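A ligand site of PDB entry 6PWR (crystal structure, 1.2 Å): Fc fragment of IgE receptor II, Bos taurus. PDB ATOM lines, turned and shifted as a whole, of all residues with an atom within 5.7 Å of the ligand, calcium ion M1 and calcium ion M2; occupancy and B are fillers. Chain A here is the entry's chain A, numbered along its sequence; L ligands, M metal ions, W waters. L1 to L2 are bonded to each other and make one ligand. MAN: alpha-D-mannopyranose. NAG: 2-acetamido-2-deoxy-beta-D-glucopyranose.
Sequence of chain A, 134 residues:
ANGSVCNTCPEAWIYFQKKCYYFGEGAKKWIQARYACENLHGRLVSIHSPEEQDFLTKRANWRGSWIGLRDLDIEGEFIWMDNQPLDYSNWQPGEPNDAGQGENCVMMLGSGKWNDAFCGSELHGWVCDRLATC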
ATOM      1  N   ARG A  63      27.195  -3.629   4.418  1.00  0.00           N
ATOM      2  CA  ARG A  63      25.956  -3.028   3.964  1.00  0.00           C
ATOM      3  C   ARG A  63      26.168  -1.880   2.984  1.00  0.00           C
ATOM      4  O   ARG A  63      25.200  -1.232   2.587  1.00  0.00           O
ATOM      5  CB  ARG A  63      25.108  -2.593   5.155  1.00  0.00           C
ATOM      6  CG  ARG A  63      24.573  -3.798   5.949  1.00  0.00           C
ATOM      7  CD  ARG A  63      23.601  -3.385   7.031  1.00  0.00           C
ATOM      8  NE  ARG A  63      24.244  -2.565   8.055  1.00  0.00           N
ATOM      9  CZ  ARG A  63      23.576  -1.876   8.968  1.00  0.00           C
ATOM     10  NH1 ARG A  63      22.245  -1.897   8.970  1.00  0.00           N
ATOM     11  NH2 ARG A  63      24.218  -1.160   9.867  1.00  0.00           N
ATOM     12  N   ASP A  71      29.174  11.907 -10.209  1.00  0.00           N
ATOM     13  CA  ASP A  71      28.986  12.590 -11.489  1.00  0.00           C
ATOM     14  C   ASP A  71      27.893  13.644 -11.362  1.00  0.00           C
ATOM     15  O   ASP A  71      27.133  13.889 -12.296  1.00  0.00           O
ATOM     16  CB  ASP A  71      28.772  11.613 -12.660  1.00  0.00           C
ATOM     17  CG  ASP A  71      27.418  10.902 -12.640  1.00  0.00           C
ATOM     18  OD1 ASP A  71      26.792  10.755 -11.571  1.00  0.00           O
ATOM     19  OD2 ASP A  71      26.945  10.471 -13.721  1.00  0.00           O
ATOM     20  N   GLU A  75      26.705  14.608 -15.942  1.00  0.00           N
ATOM     21  CA  GLU A  75      26.340  13.198 -15.955  1.00  0.00           C
ATOM     22  C   GLU A  75      27.378  12.403 -16.752  1.00  0.00           C
ATOM     23  O   GLU A  75      27.785  12.804 -17.850  1.00  0.00           O
ATOM     24  CB  GLU A  75      24.969  13.023 -16.584  1.00  0.00           C
ATOM     25  CG  GLU A  75      24.526  11.575 -16.716  1.00  0.00           C
ATOM     26  CD  GLU A  75      24.421  10.867 -15.366  1.00  0.00           C
ATOM     27  OE1 GLU A  75      24.183  11.549 -14.342  1.00  0.00           O
ATOM     28  OE2 GLU A  75      24.580   9.635 -15.343  1.00  0.00           O
ATOM     29  N   GLY A  76      27.797  11.282 -16.188  1.00  0.00           N
ATOM     30  CA  GLY A  76      28.754  10.413 -16.814  1.00  0.00           C
ATOM     31  C   GLY A  76      30.181  10.870 -16.725  1.00  0.00           C
ATOM     32  O   GLY A  76      31.079  10.154 -17.180  1.00  0.00           O
ATOM     33  N   PHE A  78      32.682  11.343 -14.037  1.00  0.00           N
ATOM     34  CA  PHE A  78      32.907  11.146 -12.620  1.00  0.00           C
ATOM     35  C   PHE A  78      34.130  11.916 -12.178  1.00  0.00           C
ATOM     36  O   PHE A  78      35.104  12.057 -12.917  1.00  0.00           O
ATOM     37  CB  PHE A  78      33.018   9.655 -12.287  1.00  0.00           C
ATOM     38  CG  PHE A  78      31.700   8.966 -12.332  1.00  0.00           C
ATOM     39  CD1 PHE A  78      31.222   8.438 -13.515  1.00  0.00           C
ATOM     40  CD2 PHE A  78      30.896   8.933 -11.215  1.00  0.00           C
ATOM     41  CE1 PHE A  78      29.986   7.843 -13.563  1.00  0.00           C
ATOM     42  CE2 PHE A  78      29.658   8.347 -11.261  1.00  0.00           C
ATOM     43  CZ  PHE A  78      29.204   7.804 -12.445  1.00  0.00           C
ATOM     44  N   GLU A  95      27.399  -1.410 -13.785  1.00  0.00           N
ATOM     45  CA  GLU A  95      27.443  -0.110 -13.169  1.00  0.00           C
ATOM     46  C   GLU A  95      28.566   0.716 -13.781  1.00  0.00           C
ATOM     47  O   GLU A  95      29.533   0.158 -14.319  1.00  0.00           O
ATOM     48  CB  GLU A  95      27.712  -0.240 -11.662  1.00  0.00           C
ATOM     49  CG  GLU A  95      26.748  -1.151 -10.940  1.00  0.00           C
ATOM     50  CD  GLU A  95      25.301  -0.708 -10.995  1.00  0.00           C
ATOM     51  OE1 GLU A  95      25.022   0.479 -11.274  1.00  0.00           O
ATOM     52  OE2 GLU A  95      24.437  -1.579 -10.747  1.00  0.00           O
ATOM     53  N   PRO A  96      28.481   2.040 -13.747  1.00  0.00           N
ATOM     54  CA  PRO A  96      27.322   2.791 -13.268  1.00  0.00           C
ATOM     55  C   PRO A  96      26.201   2.721 -14.293  1.00  0.00           C
ATOM     56  O   PRO A  96      26.464   2.689 -15.506  1.00  0.00           O
ATOM     57  CB  PRO A  96      27.866   4.218 -13.162  1.00  0.00           C
ATOM     58  CG  PRO A  96      28.935   4.273 -14.209  1.00  0.00           C
ATOM     59  CD  PRO A  96      29.556   2.917 -14.250  1.00  0.00           C
ATOM     60  N   ASN A  97      24.979   2.649 -13.809  1.00  0.00           N
ATOM     61  CA  ASN A  97      23.828   2.523 -14.684  1.00  0.00           C
ATOM     62  C   ASN A  97      22.844   3.676 -14.607  1.00  0.00           C
ATOM     63  O   ASN A  97      21.843   3.664 -15.331  1.00  0.00           O
ATOM     64  CB  ASN A  97      23.107   1.182 -14.480  1.00  0.00           C
ATOM     65  CG  ASN A  97      22.508   1.037 -13.100  1.00  0.00           C
ATOM     66  OD1 ASN A  97      22.623   1.925 -12.256  1.00  0.00           O
ATOM     67  ND2 ASN A  97      21.847  -0.085 -12.866  1.00  0.00           N
ATOM     68  N   ASP A  98      23.121   4.680 -13.774  1.00  0.00           N
ATOM     69  CA  ASP A  98      22.275   5.864 -13.626  1.00  0.00           C
ATOM     70  C   ASP A  98      20.790   5.490 -13.508  1.00  0.00           C
ATOM     71  O   ASP A  98      19.932   6.025 -14.216  1.00  0.00           O
ATOM     72  CB  ASP A  98      22.507   6.876 -14.746  1.00  0.00           C
ATOM     73  CG  ASP A  98      22.131   8.286 -14.331  1.00  0.00           C
ATOM     74  OD1 ASP A  98      22.543   8.709 -13.238  1.00  0.00           O
ATOM     75  OD2 ASP A  98      21.416   8.962 -15.099  1.00  0.00           O
ATOM     76  N   ALA A  99      20.511   4.551 -12.613  1.00  0.00           N
ATOM     77  CA  ALA A  99      19.197   3.943 -12.528  1.00  0.00           C
ATOM     78  C   ALA A  99      18.172   4.907 -11.940  1.00  0.00           C
ATOM     79  O   ALA A  99      18.498   5.952 -11.371  1.00  0.00           O
ATOM     80  CB  ALA A  99      19.250   2.669 -11.692  1.00  0.00           C
ATOM     81  N   GLY A 102      18.060   8.824 -11.517  1.00  0.00           N
ATOM     82  CA  GLY A 102      19.406   9.325 -11.663  1.00  0.00           C
ATOM     83  C   GLY A 102      20.210   8.972 -10.429  1.00  0.00           C
ATOM     84  O   GLY A 102      19.766   9.174  -9.300  1.00  0.00           O
ATOM     85  N   GLU A 103      21.390   8.419 -10.648  1.00  0.00           N
ATOM     86  CA  GLU A 103      22.275   7.991  -9.576  1.00  0.00           C
ATOM     87  C   GLU A 103      23.602   8.684  -9.817  1.00  0.00           C
ATOM     88  O   GLU A 103      24.283   8.400 -10.807  1.00  0.00           O
ATOM     89  CB  GLU A 103      22.419   6.478  -9.583  1.00  0.00           C
ATOM     90  CG  GLU A 103      21.107   5.779  -9.291  1.00  0.00           C
ATOM     91  CD  GLU A 103      21.251   4.288  -9.190  1.00  0.00           C
ATOM     92  OE1 GLU A 103      21.947   3.709 -10.036  1.00  0.00           O
ATOM     93  OE2 GLU A 103      20.683   3.688  -8.252  1.00  0.00           O
ATOM     94  N   ASN A 104      23.954   9.591  -8.926  1.00  0.00           N
ATOM     95  CA  ASN A 104      25.092  10.448  -9.181  1.00  0.00           C
ATOM     96  C   ASN A 104      26.182  10.371  -8.139  1.00  0.00           C
ATOM     97  O   ASN A 104      27.168  11.109  -8.238  1.00  0.00           O
ATOM     98  CB  ASN A 104      24.622  11.889  -9.395  1.00  0.00           C
ATOM     99  CG  ASN A 104      23.562  11.989 -10.460  1.00  0.00           C
ATOM    100  OD1 ASN A 104      23.615  11.291 -11.474  1.00  0.00           O
ATOM    101  ND2 ASN A 104      22.574  12.829 -10.224  1.00  0.00           N
ATOM    102  N   MET A 107      28.976   4.454  -4.334  1.00  0.00           N
ATOM    103  CA  MET A 107      29.208   3.670  -3.133  1.00  0.00           C
ATOM    104  C   MET A 107      30.014   2.431  -3.491  1.00  0.00           C
ATOM    105  O   MET A 107      30.053   1.974  -4.641  1.00  0.00           O
ATOM    106  CB  MET A 107      27.874   3.191  -2.529  1.00  0.00           C
ATOM    107  CG  MET A 107      27.118   2.275  -3.471  1.00  0.00           C
ATOM    108  SD  MET A 107      25.522   1.722  -2.878  1.00  0.00           S
ATOM    109  CE  MET A 107      26.000   0.706  -1.507  1.00  0.00           C
ATOM    110  N   LEU A 109      29.676  -1.433  -2.725  1.00  0.00           N
ATOM    111  CA  LEU A 109      28.843  -2.485  -2.194  1.00  0.00           C
ATOM    112  C   LEU A 109      29.607  -3.221  -1.096  1.00  0.00           C
ATOM    113  O   LEU A 109      30.790  -2.968  -0.858  1.00  0.00           O
ATOM    114  CB  LEU A 109      28.488  -3.467  -3.307  1.00  0.00           C
ATOM    115  CG  LEU A 109      27.745  -2.828  -4.475  1.00  0.00           C
ATOM    116  CD1 LEU A 109      27.555  -3.852  -5.591  1.00  0.00           C
ATOM    117  CD2 LEU A 109      26.398  -2.260  -4.053  1.00  0.00           C
ATOM    118  N   ASN A 115      29.051   0.973  -7.143  1.00  0.00           N
ATOM    119  CA  ASN A 115      27.739   1.150  -7.724  1.00  0.00           C
ATOM    120  C   ASN A 115      27.403   2.630  -7.629  1.00  0.00           C
ATOM    121  O   ASN A 115      27.633   3.247  -6.584  1.00  0.00           O
ATOM    122  CB  ASN A 115      26.723   0.365  -6.908  1.00  0.00           C
ATOM    123  CG  ASN A 115      25.307   0.662  -7.319  1.00  0.00           C
ATOM    124  OD1 ASN A 115      24.999   0.670  -8.506  1.00  0.00           O
ATOM    125  ND2 ASN A 115      24.435   0.931  -6.340  1.00  0.00           N
ATOM    126  N   ASP A 116      26.856   3.203  -8.689  1.00  0.00           N
ATOM    127  CA  ASP A 116      26.252   4.512  -8.544  1.00  0.00           C
ATOM    128  C   ASP A 116      24.893   4.382  -7.879  1.00  0.00           C
ATOM    129  O   ASP A 116      24.114   3.477  -8.175  1.00  0.00           O
ATOM    130  CB  ASP A 116      26.155   5.280  -9.869  1.00  0.00           C
ATOM    131  CG  ASP A 116      25.353   4.557 -10.950  1.00  0.00           C
ATOM    132  OD1 ASP A 116      25.152   3.328 -10.868  1.00  0.00           O
ATOM    133  OD2 ASP A 116      24.968   5.267 -11.904  1.00  0.00           O
ATOM    134  N   ALA A 117      24.618   5.293  -6.954  1.00  0.00           N
ATOM    135  CA  ALA A 117      23.382   5.251  -6.199  1.00  0.00           C
ATOM    136  C   ALA A 117      22.791   6.641  -6.137  1.00  0.00           C
ATOM    137  O   ALA A 117      23.466   7.650  -6.363  1.00  0.00           O
ATOM    138  CB  ALA A 117      23.610   4.718  -4.780  1.00  0.00           C
ATOM    139  N   PHE A 118      21.511   6.684  -5.788  1.00  0.00           N
ATOM    140  CA  PHE A 118      20.856   7.944  -5.503  1.00  0.00           C
ATOM    141  C   PHE A 118      21.593   8.640  -4.363  1.00  0.00           C
ATOM    142  O   PHE A 118      21.821   8.059  -3.304  1.00  0.00           O
ATOM    143  CB  PHE A 118      19.412   7.676  -5.112  1.00  0.00           C
ATOM    144  CG  PHE A 118      18.685   8.872  -4.581  1.00  0.00           C
ATOM    145  CD1 PHE A 118      18.742  10.085  -5.224  1.00  0.00           C
ATOM    146  CD2 PHE A 118      17.932   8.770  -3.422  1.00  0.00           C
ATOM    147  CE1 PHE A 118      18.050  11.191  -4.728  1.00  0.00           C
ATOM    148  CE2 PHE A 118      17.254   9.858  -2.919  1.00  0.00           C
ATOM    149  CZ  PHE A 118      17.324  11.066  -3.572  1.00  0.00           C
ATOM    150  N   SER A 121      20.198   8.351  -0.872  1.00  0.00           N
ATOM    151  CA  SER A 121      20.101   7.106  -0.117  1.00  0.00           C
ATOM    152  C   SER A 121      20.925   7.233   1.158  1.00  0.00           C
ATOM    153  O   SER A 121      21.910   7.973   1.213  1.00  0.00           O
ATOM    154  CB  SER A 121      20.644   5.937  -0.927  1.00  0.00           C
ATOM    155  OG  SER A 121      19.769   5.620  -1.980  1.00  0.00           O
ATOM    156  N   LEU A 123      23.318   5.316   3.652  1.00  0.00           N
ATOM    157  CA  LEU A 123      24.182   4.169   3.831  1.00  0.00           C
ATOM    158  C   LEU A 123      24.806   4.246   5.210  1.00  0.00           C
ATOM    159  O   LEU A 123      25.059   5.324   5.728  1.00  0.00           O
ATOM    160  CB  LEU A 123      25.301   4.130   2.791  1.00  0.00           C
ATOM    161  CG  LEU A 123      24.819   4.017   1.345  1.00  0.00           C
ATOM    162  CD1 LEU A 123      25.996   3.973   0.412  1.00  0.00           C
ATOM    163  CD2 LEU A 123      23.951   2.782   1.177  1.00  0.00           C
HETATM  164  C1  MAN L   1      19.643  -1.335  -7.048  1.00  0.00           C
HETATM  165  C2  MAN L   1      20.511  -0.076  -6.844  1.00  0.00           C
HETATM  166  C3  MAN L   1      21.076   0.378  -8.182  1.00  0.00           C
HETATM  167  C4  MAN L   1      21.816  -0.748  -8.841  1.00  0.00           C
HETATM  168  C5  MAN L   1      20.859  -1.921  -9.066  1.00  0.00           C
HETATM  169  C6  MAN L   1      21.548  -3.121  -9.684  1.00  0.00           C
HETATM  170  O1  MAN L   1      18.491  -0.905  -7.703  1.00  0.00           O
HETATM  171  O2  MAN L   1      21.651  -0.421  -6.099  1.00  0.00           O
HETATM  172  O3  MAN L   1      21.970   1.467  -8.042  1.00  0.00           O
HETATM  173  O4  MAN L   1      22.346  -0.302 -10.072  1.00  0.00           O
HETATM  174  O5  MAN L   1      20.334  -2.336  -7.777  1.00  0.00           O
HETATM  175  O6  MAN L   1      20.568  -4.142  -9.910  1.00  0.00           O
HETATM  176  C1  NAG L   2      21.413  -0.386  -4.698  1.00  0.00           C
HETATM  177  C2  NAG L   2      22.420  -1.324  -4.040  1.00  0.00           C
HETATM  178  C3  NAG L   2      22.247  -1.283  -2.529  1.00  0.00           C
HETATM  179  C4  NAG L   2      22.285   0.163  -2.026  1.00  0.00           C
HETATM  180  C5  NAG L   2      21.340   1.049  -2.823  1.00  0.00           C
HETATM  181  C6  NAG L   2      21.491   2.511  -2.480  1.00  0.00           C
HETATM  182  C7  NAG L   2      22.989  -3.157  -5.583  1.00  0.00           C
HETATM  183  C8  NAG L   2      22.712  -4.579  -5.970  1.00  0.00           C
HETATM  184  N2  NAG L   2      22.279  -2.680  -4.544  1.00  0.00           N
HETATM  185  O3  NAG L   2      23.299  -2.021  -1.927  1.00  0.00           O
HETATM  186  O4  NAG L   2      21.898   0.189  -0.662  1.00  0.00           O
HETATM  187  O5  NAG L   2      21.609   0.928  -4.229  1.00  0.00           O
HETATM  188  O6  NAG L   2      20.479   3.302  -3.088  1.00  0.00           O
HETATM  189  O7  NAG L   2      23.828  -2.472  -6.159  1.00  0.00           O
HETATM  190 CA    CA M   1      23.501   1.908  -9.969  1.00  0.00          CA
HETATM  191 CA    CA M   2      24.784   9.669 -12.833  1.00  0.00          CA
HETATM  192  O   HOH W   1      17.377   0.390  -9.692  1.00  0.00           O
HETATM  193  O   HOH W   2      18.798  -5.105  -7.808  1.00  0.00           O
HETATM  194  O   HOH W   3      16.245  -2.205  -7.246  1.00  0.00           O
HETATM  195  O   HOH W   4      20.006   4.199  -5.613  1.00  0.00           O
HETATM  196  O   HOH W   5      25.083  -3.142  -8.459  1.00  0.00           O
HETATM  197  O   HOH W   6      24.091  -4.708  -2.520  1.00  0.00           O
HETATM  198  O   HOH W   7      22.318  -5.625 -12.303  1.00  0.00           O
HETATM  199  O   HOH W   8      20.696  -4.323  -2.978  1.00  0.00           O
HETATM  200  O   HOH W   9      22.543  -2.909   0.636  1.00  0.00           O
HETATM  201  O   HOH W  10      25.720   7.532 -13.204  1.00  0.00           O
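Calcium ion M2 is bound by water W10 (2.4 Å), OD1 of Asn 104 (2.4 Å), O of Glu 103 (2.4 Å), OD2 of Asp 71 (2.5 Å), OD1 of Asp 98 (2.5 Å), OE1 of Glu 75 (2.5 Å), OE2 of Glu 75 (2.5 Å) and OD1 of Asp 71 (2.6 Å).
Calcium ion M1 is bound by the side-chain carboxylate (OD1) of Asp 116 (2.4 Å), the side-chain carboxylate (OE1) of Glu 103 (2.4 Å), the side-chain amide oxygen (OD1) of Asn 115 (2.4 Å), the side-chain amide oxygen (OD1) of Asn 97 (2.4 Å), the side-chain carboxylate (OE1) of Glu 95 (2.5 Å), the backbone carbonyl oxygen (O) of Asp 116 (2.5 Å), an oxygen (O4) of MAN L1 (2.5 Å) and an oxygen (O3) of MAN L1 (2.5 Å). Calcium ion M1 has eight donor atoms within binding distance.
The nearest printed residue that does not touch calcium ion M1 is Ala 99 (4.6 Å).
The side-chain hydroxyl of Ser 121 lies within hydrogen-bond range of an oxygen (O6) of NAG L2 (2.7 Å).
Five residues have an atom within 4 Å of calcium ion M2: Asp 71, Glu 75, Asp 98, Glu 103 and Asn 104.
Met 107 touches the ligand. Leu 109 touches the ligand. Ala 117 touches the ligand. Leu 123 touches the ligand. Hydrophobic or aromatic side chains within 4 Å of the ligand: Met 107, Leu 109, Ala 117 and Leu 123. Ten residues have an atom within 4 Å of the ligand: Glu 95, Asn 97, Glu 103, Met 107, Leu 109, Asn 115, Asp 116, Ala 117, Ser 121 and Leu 123. The nearest printed residue that does not touch the ligand is Phe 118 (4.4 Å).
O of Phe 118 sits close to OG of Ser 121, 3.5 Å away. OD2 of Asp 71 lies close to N of Gly 76 (2.7 Å). The backbone carbonyl oxygen (O) of Met 107 is in hydrogen-bond range of the backbone NH (N) of Asn 115 (2.9 Å). The backbone carbonyl oxygen (O) of Ala 117 lies within hydrogen-bond range of the backbone NH (N) of Asn 104. OD1 of Asn 97 sits close to N of Ala 99, at 3.4 Å. The side-chain carboxylate (OD2) of Asp 116 sits at hydrogen-bond distance from the backbone NH (N) of Asp 98 (2.7 Å). OE1 of Glu 103 sits close to N of Ala 99.
Water W5 bridges O7 of NAG L2 and OE2 of Glu 95. Water W4 lies within hydrogen-bond range of O6 of NAG L2 (2.7 Å), OE2 of Glu 103 (2.8 Å) and N of Phe 118 (2.9 Å).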
